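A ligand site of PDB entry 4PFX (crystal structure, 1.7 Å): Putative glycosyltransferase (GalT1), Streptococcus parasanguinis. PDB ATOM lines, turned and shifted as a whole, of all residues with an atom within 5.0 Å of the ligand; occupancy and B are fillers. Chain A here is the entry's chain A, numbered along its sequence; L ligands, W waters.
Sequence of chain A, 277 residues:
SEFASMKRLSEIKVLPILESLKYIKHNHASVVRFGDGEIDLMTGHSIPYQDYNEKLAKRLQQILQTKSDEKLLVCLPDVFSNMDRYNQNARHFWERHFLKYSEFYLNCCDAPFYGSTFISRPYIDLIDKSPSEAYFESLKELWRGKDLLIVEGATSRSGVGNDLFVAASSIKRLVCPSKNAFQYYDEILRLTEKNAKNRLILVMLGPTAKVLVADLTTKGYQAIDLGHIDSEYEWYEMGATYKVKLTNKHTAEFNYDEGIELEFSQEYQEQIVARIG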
ATOM      1  N   ARG A  33     -17.002 -17.811 -13.931  1.00  0.00           N
ATOM      2  CA  ARG A  33     -15.895 -18.727 -14.172  1.00  0.00           C
ATOM      3  C   ARG A  33     -15.480 -18.696 -15.628  1.00  0.00           C
ATOM      4  O   ARG A  33     -16.318 -18.778 -16.529  1.00  0.00           O
ATOM      5  CB  ARG A  33     -16.297 -20.160 -13.786  1.00  0.00           C
ATOM      6  CG  ARG A  33     -16.742 -20.357 -12.329  1.00  0.00           C
ATOM      7  CD  ARG A  33     -17.229 -21.800 -12.066  1.00  0.00           C
ATOM      8  NE  ARG A  33     -18.266 -22.102 -13.035  1.00  0.00           N
ATOM      9  CZ  ARG A  33     -18.073 -22.778 -14.165  1.00  0.00           C
ATOM     10  NH1 ARG A  33     -16.906 -23.361 -14.422  1.00  0.00           N
ATOM     11  NH2 ARG A  33     -19.087 -22.884 -15.007  1.00  0.00           N
ATOM     12  N   GLU A  38     -14.404 -20.413 -22.936  1.00  0.00           N
ATOM     13  CA  GLU A  38     -14.451 -18.957 -22.913  1.00  0.00           C
ATOM     14  C   GLU A  38     -13.237 -18.351 -23.592  1.00  0.00           C
ATOM     15  O   GLU A  38     -13.344 -17.367 -24.324  1.00  0.00           O
ATOM     16  CB  GLU A  38     -14.581 -18.409 -21.487  1.00  0.00           C
ATOM     17  CG  GLU A  38     -16.002 -18.597 -20.909  1.00  0.00           C
ATOM     18  CD  GLU A  38     -16.398 -20.069 -20.814  1.00  0.00           C
ATOM     19  OE1 GLU A  38     -15.657 -20.856 -20.175  1.00  0.00           O
ATOM     20  OE2 GLU A  38     -17.449 -20.436 -21.388  1.00  0.00           O
ATOM     21  N   TYR A  49     -21.343 -25.922 -27.719  1.00  0.00           N
ATOM     22  CA  TYR A  49     -22.673 -25.379 -27.473  1.00  0.00           C
ATOM     23  C   TYR A  49     -22.811 -23.868 -27.573  1.00  0.00           C
ATOM     24  O   TYR A  49     -23.766 -23.295 -27.073  1.00  0.00           O
ATOM     25  CB  TYR A  49     -23.302 -25.877 -26.140  1.00  0.00           C
ATOM     26  CG  TYR A  49     -22.413 -25.968 -24.910  1.00  0.00           C
ATOM     27  CD1 TYR A  49     -21.677 -24.872 -24.449  1.00  0.00           C
ATOM     28  CD2 TYR A  49     -22.359 -27.138 -24.172  1.00  0.00           C
ATOM     29  CE1 TYR A  49     -20.878 -24.974 -23.300  1.00  0.00           C
ATOM     30  CE2 TYR A  49     -21.583 -27.260 -23.033  1.00  0.00           C
ATOM     31  CZ  TYR A  49     -20.839 -26.168 -22.593  1.00  0.00           C
ATOM     32  OH  TYR A  49     -20.074 -26.330 -21.469  1.00  0.00           O
ATOM     33  N   GLN A  50     -21.862 -23.224 -28.243  1.00  0.00           N
ATOM     34  CA  GLN A  50     -21.962 -21.789 -28.504  1.00  0.00           C
ATOM     35  C   GLN A  50     -21.103 -21.355 -29.678  1.00  0.00           C
ATOM     36  O   GLN A  50     -19.873 -21.387 -29.613  1.00  0.00           O
ATOM     37  CB  GLN A  50     -21.617 -20.979 -27.243  1.00  0.00           C
ATOM     38  CG  GLN A  50     -21.679 -19.464 -27.456  1.00  0.00           C
ATOM     39  CD  GLN A  50     -23.074 -18.987 -27.829  1.00  0.00           C
ATOM     40  OE1 GLN A  50     -24.009 -19.196 -27.072  1.00  0.00           O
ATOM     41  NE2 GLN A  50     -23.195 -18.364 -29.004  1.00  0.00           N
ATOM     42  N   THR A 117     -12.174 -21.933 -11.406  1.00  0.00           N
ATOM     43  CA  THR A 117     -13.201 -22.346 -12.341  1.00  0.00           C
ATOM     44  C   THR A 117     -13.689 -23.759 -12.006  1.00  0.00           C
ATOM     45  O   THR A 117     -14.782 -24.173 -12.421  1.00  0.00           O
ATOM     46  CB  THR A 117     -12.623 -22.228 -13.757  1.00  0.00           C
ATOM     47  OG1 THR A 117     -12.503 -20.840 -14.081  1.00  0.00           O
ATOM     48  CG2 THR A 117     -13.492 -22.927 -14.800  1.00  0.00           C
ATOM     49  N   SER A 120     -17.124 -25.889 -10.076  1.00  0.00           N
ATOM     50  CA  SER A 120     -18.169 -26.709 -10.707  1.00  0.00           C
ATOM     51  C   SER A 120     -17.654 -28.079 -11.112  1.00  0.00           C
ATOM     52  O   SER A 120     -18.438 -28.912 -11.573  1.00  0.00           O
ATOM     53  CB  SER A 120     -18.691 -26.050 -11.973  1.00  0.00           C
ATOM     54  OG  SER A 120     -17.636 -25.866 -12.889  1.00  0.00           O
ATOM     55  N   ARG A 121     -16.348 -28.303 -10.957  1.00  0.00           N
ATOM     56  CA  ARG A 121     -15.713 -29.527 -11.460  1.00  0.00           C
ATOM     57  C   ARG A 121     -14.889 -30.185 -10.361  1.00  0.00           C
ATOM     58  O   ARG A 121     -13.658 -30.242 -10.431  1.00  0.00           O
ATOM     59  CB  ARG A 121     -14.821 -29.205 -12.654  1.00  0.00           C
ATOM     60  CG  ARG A 121     -15.448 -28.297 -13.720  1.00  0.00           C
ATOM     61  CD  ARG A 121     -16.676 -28.927 -14.360  1.00  0.00           C
ATOM     62  NE  ARG A 121     -16.389 -30.266 -14.852  1.00  0.00           N
ATOM     63  CZ  ARG A 121     -16.420 -30.645 -16.129  1.00  0.00           C
ATOM     64  NH1 ARG A 121     -16.772 -29.794 -17.074  1.00  0.00           N
ATOM     65  NH2 ARG A 121     -16.132 -31.902 -16.442  1.00  0.00           N
ATOM     66  N   GLU A 152     -30.794 -22.247 -16.645  1.00  0.00           N
ATOM     67  CA  GLU A 152     -30.013 -23.348 -17.223  1.00  0.00           C
ATOM     68  C   GLU A 152     -30.641 -23.733 -18.570  1.00  0.00           C
ATOM     69  O   GLU A 152     -31.707 -23.243 -18.922  1.00  0.00           O
ATOM     70  CB  GLU A 152     -30.027 -24.573 -16.302  1.00  0.00           C
ATOM     71  CG  GLU A 152     -31.422 -25.195 -16.126  1.00  0.00           C
ATOM     72  CD  GLU A 152     -31.463 -26.423 -15.229  1.00  0.00           C
ATOM     73  OE1 GLU A 152     -30.407 -26.859 -14.706  1.00  0.00           O
ATOM     74  OE2 GLU A 152     -32.576 -26.956 -15.051  1.00  0.00           O
ATOM     75  N   GLY A 153     -29.982 -24.626 -19.292  1.00  0.00           N
ATOM     76  CA  GLY A 153     -30.492 -25.083 -20.570  1.00  0.00           C
ATOM     77  C   GLY A 153     -31.501 -26.202 -20.485  1.00  0.00           C
ATOM     78  O   GLY A 153     -31.670 -26.833 -19.433  1.00  0.00           O
ATOM     79  N   ALA A 154     -32.153 -26.465 -21.611  1.00  0.00           N
ATOM     80  CA  ALA A 154     -33.221 -27.460 -21.693  1.00  0.00           C
ATOM     81  C   ALA A 154     -32.766 -28.873 -21.330  1.00  0.00           C
ATOM     82  O   ALA A 154     -33.561 -29.678 -20.838  1.00  0.00           O
ATOM     83  CB  ALA A 154     -33.888 -27.435 -23.078  1.00  0.00           C
ATOM     84  N   THR A 155     -31.486 -29.178 -21.563  1.00  0.00           N
ATOM     85  CA  THR A 155     -30.970 -30.506 -21.241  1.00  0.00           C
ATOM     86  C   THR A 155     -30.150 -30.551 -19.939  1.00  0.00           C
ATOM     87  O   THR A 155     -29.766 -31.629 -19.492  1.00  0.00           O
ATOM     88  CB  THR A 155     -30.111 -31.082 -22.384  1.00  0.00           C
ATOM     89  OG1 THR A 155     -28.945 -30.260 -22.573  1.00  0.00           O
ATOM     90  CG2 THR A 155     -30.907 -31.144 -23.672  1.00  0.00           C
ATOM     91  N   SER A 156     -29.917 -29.392 -19.317  1.00  0.00           N
ATOM     92  CA  SER A 156     -29.063 -29.326 -18.130  1.00  0.00           C
ATOM     93  C   SER A 156     -29.668 -30.103 -16.964  1.00  0.00           C
ATOM     94  O   SER A 156     -28.993 -30.893 -16.310  1.00  0.00           O
ATOM     95  CB  SER A 156     -28.828 -27.860 -17.701  1.00  0.00           C
ATOM     96  OG  SER A 156     -28.181 -27.116 -18.728  1.00  0.00           O
ATOM     97  N   PRO A 177     -32.164 -22.167 -24.149  1.00  0.00           N
ATOM     98  CA  PRO A 177     -31.669 -23.121 -25.160  1.00  0.00           C
ATOM     99  C   PRO A 177     -30.429 -23.870 -24.673  1.00  0.00           C
ATOM    100  O   PRO A 177     -29.597 -23.297 -23.984  1.00  0.00           O
ATOM    101  CB  PRO A 177     -31.314 -22.217 -26.343  1.00  0.00           C
ATOM    102  CG  PRO A 177     -32.153 -21.007 -26.167  1.00  0.00           C
ATOM    103  CD  PRO A 177     -32.272 -20.799 -24.683  1.00  0.00           C
ATOM    104  N   SER A 178     -30.325 -25.131 -25.055  1.00  0.00           N
ATOM    105  CA  SER A 178     -29.197 -25.952 -24.631  1.00  0.00           C
ATOM    106  C   SER A 178     -27.908 -25.608 -25.392  1.00  0.00           C
ATOM    107  O   SER A 178     -26.816 -25.974 -24.970  1.00  0.00           O
ATOM    108  CB  SER A 178     -29.530 -27.432 -24.808  1.00  0.00           C
ATOM    109  OG  SER A 178     -29.863 -27.701 -26.157  1.00  0.00           O
ATOM    110  N   LYS A 179     -28.056 -24.920 -26.511  1.00  0.00           N
ATOM    111  CA  LYS A 179     -26.922 -24.431 -27.285  1.00  0.00           C
ATOM    112  C   LYS A 179     -27.256 -23.043 -27.821  1.00  0.00           C
ATOM    113  O   LYS A 179     -28.427 -22.735 -28.067  1.00  0.00           O
ATOM    114  CB  LYS A 179     -26.627 -25.354 -28.480  1.00  0.00           C
ATOM    115  CG  LYS A 179     -26.263 -26.784 -28.134  1.00  0.00           C
ATOM    116  CD  LYS A 179     -26.078 -27.604 -29.410  1.00  0.00           C
ATOM    117  CE  LYS A 179     -25.604 -29.012 -29.109  1.00  0.00           C
ATOM    118  NZ  LYS A 179     -25.454 -29.794 -30.367  1.00  0.00           N
ATOM    119  N   ASN A 180     -26.241 -22.208 -28.011  1.00  0.00           N
ATOM    120  CA  ASN A 180     -26.454 -20.891 -28.614  1.00  0.00           C
ATOM    121  C   ASN A 180     -27.441 -20.045 -27.827  1.00  0.00           C
ATOM    122  O   ASN A 180     -28.253 -19.322 -28.419  1.00  0.00           O
ATOM    123  CB  ASN A 180     -26.923 -21.035 -30.067  1.00  0.00           C
ATOM    124  CG  ASN A 180     -25.782 -21.109 -31.057  1.00  0.00           C
ATOM    125  OD1 ASN A 180     -24.622 -21.170 -30.672  1.00  0.00           O
ATOM    126  ND2 ASN A 180     -26.117 -21.094 -32.344  1.00  0.00           N
ATOM    127  N   ALA A 181     -27.375 -20.126 -26.499  1.00  0.00           N
ATOM    128  CA  ALA A 181     -28.270 -19.354 -25.669  1.00  0.00           C
ATOM    129  C   ALA A 181     -28.041 -17.851 -25.823  1.00  0.00           C
ATOM    130  O   ALA A 181     -28.951 -17.061 -25.570  1.00  0.00           O
ATOM    131  CB  ALA A 181     -28.148 -19.755 -24.206  1.00  0.00           C
ATOM    132  N   MET A 204     -26.279 -22.172 -15.078  1.00  0.00           N
ATOM    133  CA  MET A 204     -25.591 -23.267 -15.766  1.00  0.00           C
ATOM    134  C   MET A 204     -25.877 -23.094 -17.243  1.00  0.00           C
ATOM    135  O   MET A 204     -26.839 -23.657 -17.789  1.00  0.00           O
ATOM    136  CB  MET A 204     -26.099 -24.629 -15.283  1.00  0.00           C
ATOM    137  CG  MET A 204     -25.924 -24.910 -13.783  1.00  0.00           C
ATOM    138  SD  MET A 204     -27.095 -23.949 -12.744  1.00  0.00           S
ATOM    139  CE  MET A 204     -27.148 -24.997 -11.283  1.00  0.00           C
ATOM    140  N   LEU A 205     -25.062 -22.274 -17.910  1.00  0.00           N
ATOM    141  CA  LEU A 205     -25.435 -21.822 -19.235  1.00  0.00           C
ATOM    142  C   LEU A 205     -24.226 -21.457 -20.103  1.00  0.00           C
ATOM    143  O   LEU A 205     -24.284 -20.518 -20.881  1.00  0.00           O
ATOM    144  CB  LEU A 205     -26.426 -20.655 -19.119  1.00  0.00           C
ATOM    145  CG  LEU A 205     -27.370 -20.526 -20.319  1.00  0.00           C
ATOM    146  CD1 LEU A 205     -28.402 -21.635 -20.292  1.00  0.00           C
ATOM    147  CD2 LEU A 205     -28.056 -19.162 -20.337  1.00  0.00           C
ATOM    148  N   GLY A 206     -23.134 -22.208 -19.988  1.00  0.00           N
ATOM    149  CA  GLY A 206     -21.987 -21.971 -20.865  1.00  0.00           C
ATOM    150  C   GLY A 206     -21.495 -20.534 -20.843  1.00  0.00           C
ATOM    151  O   GLY A 206     -21.540 -19.873 -19.790  1.00  0.00           O
ATOM    152  N   PRO A 207     -21.008 -20.022 -21.984  1.00  0.00           N
ATOM    153  CA  PRO A 207     -20.445 -18.667 -22.055  1.00  0.00           C
ATOM    154  C   PRO A 207     -21.494 -17.617 -21.706  1.00  0.00           C
ATOM    155  O   PRO A 207     -21.150 -16.576 -21.131  1.00  0.00           O
ATOM    156  CB  PRO A 207     -20.069 -18.517 -23.535  1.00  0.00           C
ATOM    157  CG  PRO A 207     -19.879 -19.910 -24.010  1.00  0.00           C
ATOM    158  CD  PRO A 207     -20.818 -20.786 -23.229  1.00  0.00           C
ATOM    159  N   THR A 208     -22.743 -17.881 -22.077  1.00  0.00           N
ATOM    160  CA  THR A 208     -23.823 -16.950 -21.804  1.00  0.00           C
ATOM    161  C   THR A 208     -23.960 -16.693 -20.306  1.00  0.00           C
ATOM    162  O   THR A 208     -24.305 -15.567 -19.888  1.00  0.00           O
ATOM    163  CB  THR A 208     -25.156 -17.431 -22.395  1.00  0.00           C
ATOM    164  OG1 THR A 208     -24.987 -17.622 -23.796  1.00  0.00           O
ATOM    165  CG2 THR A 208     -26.270 -16.384 -22.152  1.00  0.00           C
ATOM    166  N   LYS A 210     -21.672 -16.339 -18.123  1.00  0.00           N
ATOM    167  CA  LYS A 210     -20.693 -15.383 -17.597  1.00  0.00           C
ATOM    168  C   LYS A 210     -21.206 -13.937 -17.731  1.00  0.00           C
ATOM    169  O   LYS A 210     -21.032 -13.113 -16.829  1.00  0.00           O
ATOM    170  CB  LYS A 210     -19.346 -15.516 -18.303  1.00  0.00           C
ATOM    171  CG  LYS A 210     -18.971 -16.907 -18.816  1.00  0.00           C
ATOM    172  CD  LYS A 210     -19.001 -17.960 -17.743  1.00  0.00           C
ATOM    173  CE  LYS A 210     -18.637 -19.336 -18.321  1.00  0.00           C
ATOM    174  NZ  LYS A 210     -18.992 -20.383 -17.354  1.00  0.00           N
ATOM    175  N   ASP A 225     -22.249 -18.772 -11.104  1.00  0.00           N
ATOM    176  CA  ASP A 225     -21.998 -19.588 -12.287  1.00  0.00           C
ATOM    177  C   ASP A 225     -21.555 -20.998 -11.862  1.00  0.00           C
ATOM    178  O   ASP A 225     -20.408 -21.182 -11.395  1.00  0.00           O
ATOM    179  CB  ASP A 225     -20.960 -18.857 -13.124  1.00  0.00           C
ATOM    180  CG  ASP A 225     -20.437 -19.678 -14.300  1.00  0.00           C
ATOM    181  OD1 ASP A 225     -21.004 -20.726 -14.629  1.00  0.00           O
ATOM    182  OD2 ASP A 225     -19.434 -19.222 -14.890  1.00  0.00           O
ATOM    183  N   LEU A 226     -22.461 -21.973 -11.983  1.00  0.00           N
ATOM    184  CA  LEU A 226     -22.170 -23.345 -11.530  1.00  0.00           C
ATOM    185  C   LEU A 226     -22.020 -24.367 -12.649  1.00  0.00           C
ATOM    186  O   LEU A 226     -21.780 -25.534 -12.361  1.00  0.00           O
ATOM    187  CB  LEU A 226     -23.221 -23.842 -10.548  1.00  0.00           C
ATOM    188  CG  LEU A 226     -23.175 -23.154  -9.193  1.00  0.00           C
ATOM    189  CD1 LEU A 226     -24.223 -23.808  -8.292  1.00  0.00           C
ATOM    190  CD2 LEU A 226     -21.779 -23.290  -8.593  1.00  0.00           C
ATOM    191  N   GLY A 227     -22.200 -23.945 -13.891  1.00  0.00           N
ATOM    192  CA  GLY A 227     -21.826 -24.783 -15.033  1.00  0.00           C
ATOM    193  C   GLY A 227     -22.212 -26.246 -14.966  1.00  0.00           C
ATOM    194  O   GLY A 227     -23.397 -26.591 -14.870  1.00  0.00           O
ATOM    195  N   HIS A 228     -21.209 -27.125 -15.040  1.00  0.00           N
ATOM    196  CA  HIS A 228     -21.462 -28.561 -15.122  1.00  0.00           C
ATOM    197  C   HIS A 228     -21.514 -29.295 -13.783  1.00  0.00           C
ATOM    198  O   HIS A 228     -21.282 -30.523 -13.710  1.00  0.00           O
ATOM    199  CB  HIS A 228     -20.389 -29.199 -16.002  1.00  0.00           C
ATOM    200  CG  HIS A 228     -20.698 -29.160 -17.463  1.00  0.00           C
ATOM    201  ND1 HIS A 228     -19.837 -28.625 -18.394  1.00  0.00           N
ATOM    202  CD2 HIS A 228     -21.769 -29.626 -18.161  1.00  0.00           C
ATOM    203  CE1 HIS A 228     -20.382 -28.723 -19.598  1.00  0.00           C
ATOM    204  NE2 HIS A 228     -21.538 -29.355 -19.490  1.00  0.00           N
ATOM    205  N   ILE A 229     -21.808 -28.561 -12.712  1.00  0.00           N
ATOM    206  CA  ILE A 229     -21.878 -29.181 -11.387  1.00  0.00           C
ATOM    207  C   ILE A 229     -22.713 -30.465 -11.350  1.00  0.00           C
ATOM    208  O   ILE A 229     -22.355 -31.408 -10.661  1.00  0.00           O
ATOM    209  CB  ILE A 229     -22.344 -28.168 -10.294  1.00  0.00           C
ATOM    210  CG1 ILE A 229     -22.159 -28.773  -8.899  1.00  0.00           C
ATOM    211  CG2 ILE A 229     -23.792 -27.729 -10.510  1.00  0.00           C
ATOM    212  CD1 ILE A 229     -20.733 -29.140  -8.613  1.00  0.00           C
ATOM    213  N   HIS A 250     -28.222 -33.903 -20.282  1.00  0.00           N
ATOM    214  CA  HIS A 250     -26.896 -33.482 -20.703  1.00  0.00           C
ATOM    215  C   HIS A 250     -25.790 -34.079 -19.829  1.00  0.00           C
ATOM    216  O   HIS A 250     -25.957 -34.187 -18.604  1.00  0.00           O
ATOM    217  CB  HIS A 250     -26.817 -31.955 -20.588  1.00  0.00           C
ATOM    218  CG  HIS A 250     -25.483 -31.373 -20.919  1.00  0.00           C
ATOM    219  ND1 HIS A 250     -25.017 -31.270 -22.219  1.00  0.00           N
ATOM    220  CD2 HIS A 250     -24.500 -30.860 -20.137  1.00  0.00           C
ATOM    221  CE1 HIS A 250     -23.819 -30.732 -22.211  1.00  0.00           C
ATOM    222  NE2 HIS A 250     -23.470 -30.477 -20.960  1.00  0.00           N
ATOM    223  N   GLU A 253     -18.983 -32.571 -21.442  1.00  0.00           N
ATOM    224  CA  GLU A 253     -18.038 -33.046 -22.475  1.00  0.00           C
ATOM    225  C   GLU A 253     -18.619 -34.083 -23.452  1.00  0.00           C
ATOM    226  O   GLU A 253     -17.893 -34.666 -24.260  1.00  0.00           O
ATOM    227  CB  GLU A 253     -16.708 -33.498 -21.859  1.00  0.00           C
ATOM    228  CG  GLU A 253     -15.854 -32.316 -21.384  1.00  0.00           C
ATOM    229  CD  GLU A 253     -16.217 -31.865 -19.984  1.00  0.00           C
ATOM    230  OE1 GLU A 253     -16.019 -32.661 -19.054  1.00  0.00           O
ATOM    231  OE2 GLU A 253     -16.708 -30.716 -19.830  1.00  0.00           O
HETATM  232  N1  LIG L   1     -25.446 -24.698 -21.630  1.00  0.00           N
HETATM  233  C1  LIG L   1     -26.719 -24.359 -22.057  1.00  0.00           C
HETATM  234  N2  LIG L   1     -26.877 -23.528 -23.139  1.00  0.00           N
HETATM  235  C2  LIG L   1     -25.783 -22.996 -23.796  1.00  0.00           C
HETATM  236  C3  LIG L   1     -24.510 -23.335 -23.369  1.00  0.00           C
HETATM  237  C4  LIG L   1     -24.362 -24.291 -22.354  1.00  0.00           C
HETATM  238  O1  LIG L   1     -27.698 -24.820 -21.472  1.00  0.00           O
HETATM  239  O2  LIG L   1     -25.951 -22.245 -24.759  1.00  0.00           O
HETATM  240  C5  LIG L   1     -25.296 -25.523 -20.420  1.00  0.00           C
HETATM  241  C6  LIG L   1     -24.887 -26.964 -20.561  1.00  0.00           C
HETATM  242  O3  LIG L   1     -26.009 -27.756 -20.886  1.00  0.00           O
HETATM  243  C7  LIG L   1     -24.401 -27.221 -19.141  1.00  0.00           C
HETATM  244  C8  LIG L   1     -23.780 -25.895 -18.724  1.00  0.00           C
HETATM  245  O4  LIG L   1     -24.269 -24.930 -19.647  1.00  0.00           O
HETATM  246  O5  LIG L   1     -25.501 -27.505 -18.282  1.00  0.00           O
HETATM  247  C9  LIG L   1     -22.260 -25.928 -18.713  1.00  0.00           C
HETATM  248  O6  LIG L   1     -21.768 -24.614 -18.459  1.00  0.00           O
HETATM  249  P1  LIG L   1     -20.198 -24.285 -18.415  1.00  0.00           P
HETATM  250  O7  LIG L   1     -19.634 -24.389 -19.779  1.00  0.00           O
HETATM  251  O8  LIG L   1     -20.060 -22.956 -17.764  1.00  0.00           O
HETATM  252  O9  LIG L   1     -19.713 -25.487 -17.483  1.00  0.00           O
HETATM  253  P2  LIG L   1     -18.269 -25.850 -16.860  1.00  0.00           P
HETATM  254  O10 LIG L   1     -17.732 -27.041 -17.587  1.00  0.00           O
HETATM  255  O11 LIG L   1     -18.529 -26.207 -15.458  1.00  0.00           O
HETATM  256  O12 LIG L   1     -17.303 -24.720 -16.979  1.00  0.00           O
HETATM  257  O   HOH W   1     -18.508 -22.890 -21.680  1.00  0.00           O
HETATM  258  O   HOH W   2     -16.665 -21.984 -17.721  1.00  0.00           O
HETATM  259  O   HOH W   3     -24.840 -29.433 -16.562  1.00  0.00           O
HETATM  260  O   HOH W   4     -25.892 -28.072 -23.546  1.00  0.00           O
HETATM  261  O   HOH W   5     -22.493 -21.946 -16.587  1.00  0.00           O
HETATM  262  O   HOH W   6     -28.912 -27.666 -21.696  1.00  0.00           O
HETATM  263  O   HOH W   7     -24.030 -19.981 -24.443  1.00  0.00           O
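OG of Ser 120 lies within hydrogen-bond range of NH1 of Arg 33, at 3.0 Å. The side-chain hydroxyl of Ser 120 sits at hydrogen-bond distance from the backbone carbonyl oxygen of Thr 117, at 3.4 Å. The side-chain hydroxyl of Ser 156 is in hydrogen-bond range of the backbone NH of Gly 153 (3.1 Å). The side-chain amino group (NZ) of Lys 210 lies close to the backbone carbonyl oxygen (O) of Arg 33 (3.2 Å). NZ of Lys 210 lies within salt-bridge range of OD2 of Asp 225. The guanidinium group (NH2) of Arg 33 lies within salt-bridge range of the side-chain carboxylate (OD1) of Asp 225 (2.9 Å). OE1 of Glu 253 lies within salt-bridge range of NH2 of Arg 121, at 2.7 Å. N of His 250 sits at hydrogen-bond distance from O of Thr 155, at 2.9 Å.
Water W1 bridges an oxygen (O7) of the ligand (2.7 Å) and the side-chain carboxylate (OE2) of Glu 38 (2.7 Å). Water W4 bridges an oxygen (O3) of the ligand and the backbone carbonyl oxygen of Ser 178. Water W2 lies within hydrogen-bond range of the side-chain amino group of Lys 210 (2.8 Å), the side-chain carboxylate of Glu 38 (2.9 Å), an oxygen (O12) of the ligand (2.9 Å) and the backbone carbonyl oxygen of Arg 33 (3.4 Å). Water W7 lies within hydrogen-bond range of OG1 of Thr 208 (2.6 Å), OE1 of Gln 50 (2.7 Å) and O2 of the ligand (3.0 Å). Water W6 lies within hydrogen-bond range of the side-chain hydroxyl (OG1) of Thr 155 (2.7 Å), an oxygen (O3) of the ligand (3.0 Å), the side-chain hydroxyl (OG) of Ser 156 (3.1 Å) and the backbone NH (N) of Ala 154 (3.5 Å).
O of Met 204 lies close to O4 of the ligand. C of Lys 179 touches O2 of the ligand, 3.4 Å away. OD1 of Asp 225 touches O8 of the ligand, 3.96 Å away. Gly 227 touches the ligand (CA to O9, 3.3 Å). CD2 of His 250 touches O3 of the ligand, at 3.5 Å. Hydrophobic or aromatic side chains that line the ligand: Tyr 49, Ala 181, Leu 205, His 228 and His 250. 19 residues have an atom within 4 Å of the ligand: Arg 33, Tyr 49, Ser 120, Arg 121, Gly 153, Ser 156, Pro 177, Ser 178, Lys 179, Asn 180, Ala 181, Met 204, Leu 205, Gly 206, Lys 210, Asp 225, Gly 227, His 228 and His 250.
The side-chain hydroxyl (OH) of Tyr 49 lies within hydrogen-bond range of an oxygen (O7) of the ligand (2.6 Å). An oxygen (O11) of the ligand sits at hydrogen-bond distance from the side-chain hydroxyl of Ser 120 (2.7 Å). An oxygen (O5) of the ligand lies within hydrogen-bond range of the side-chain hydroxyl of Ser 156 (2.7 Å). O11 of the ligand lies within hydrogen-bond range of N of His 228 (2.9 Å). A ring nitrogen (ND1) of His 228 sits at hydrogen-bond distance from an oxygen (O10) of the ligand, 2.8 Å away. The side-chain amino group (NZ) of Lys 210 lies within salt-bridge range of an oxygen (O8) of the ligand (2.8 Å). N2 of the ligand sits at hydrogen-bond distance from O of Pro 177, 2.9 Å away. The guanidinium group (NH1) of Arg 33 lies within salt-bridge range of an oxygen (O12) of the ligand, at 2.9 Å. The backbone NH of Gly 153 lies close to an oxygen (O1) of the ligand (3.2 Å). O10 of the ligand is in salt-bridge range of NH1 of Arg 121 (3.0 Å). N of Gly 206 is in hydrogen-bond range of O4 of the ligand, 3.0 Å away. The backbone carbonyl oxygen (O) of Ser 178 sits at hydrogen-bond distance from a nitrogen (N2) of the ligand (3.1 Å). The backbone NH of Ala 181 sits at hydrogen-bond distance from an oxygen (O2) of the ligand (3.1 Å). The backbone NH (N) of Asn 180 sits at hydrogen-bond distance from an oxygen (O2) of the ligand, at 3.3 Å. N of Leu 205 sits at hydrogen-bond distance from O4 of the ligand (3.3 Å).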
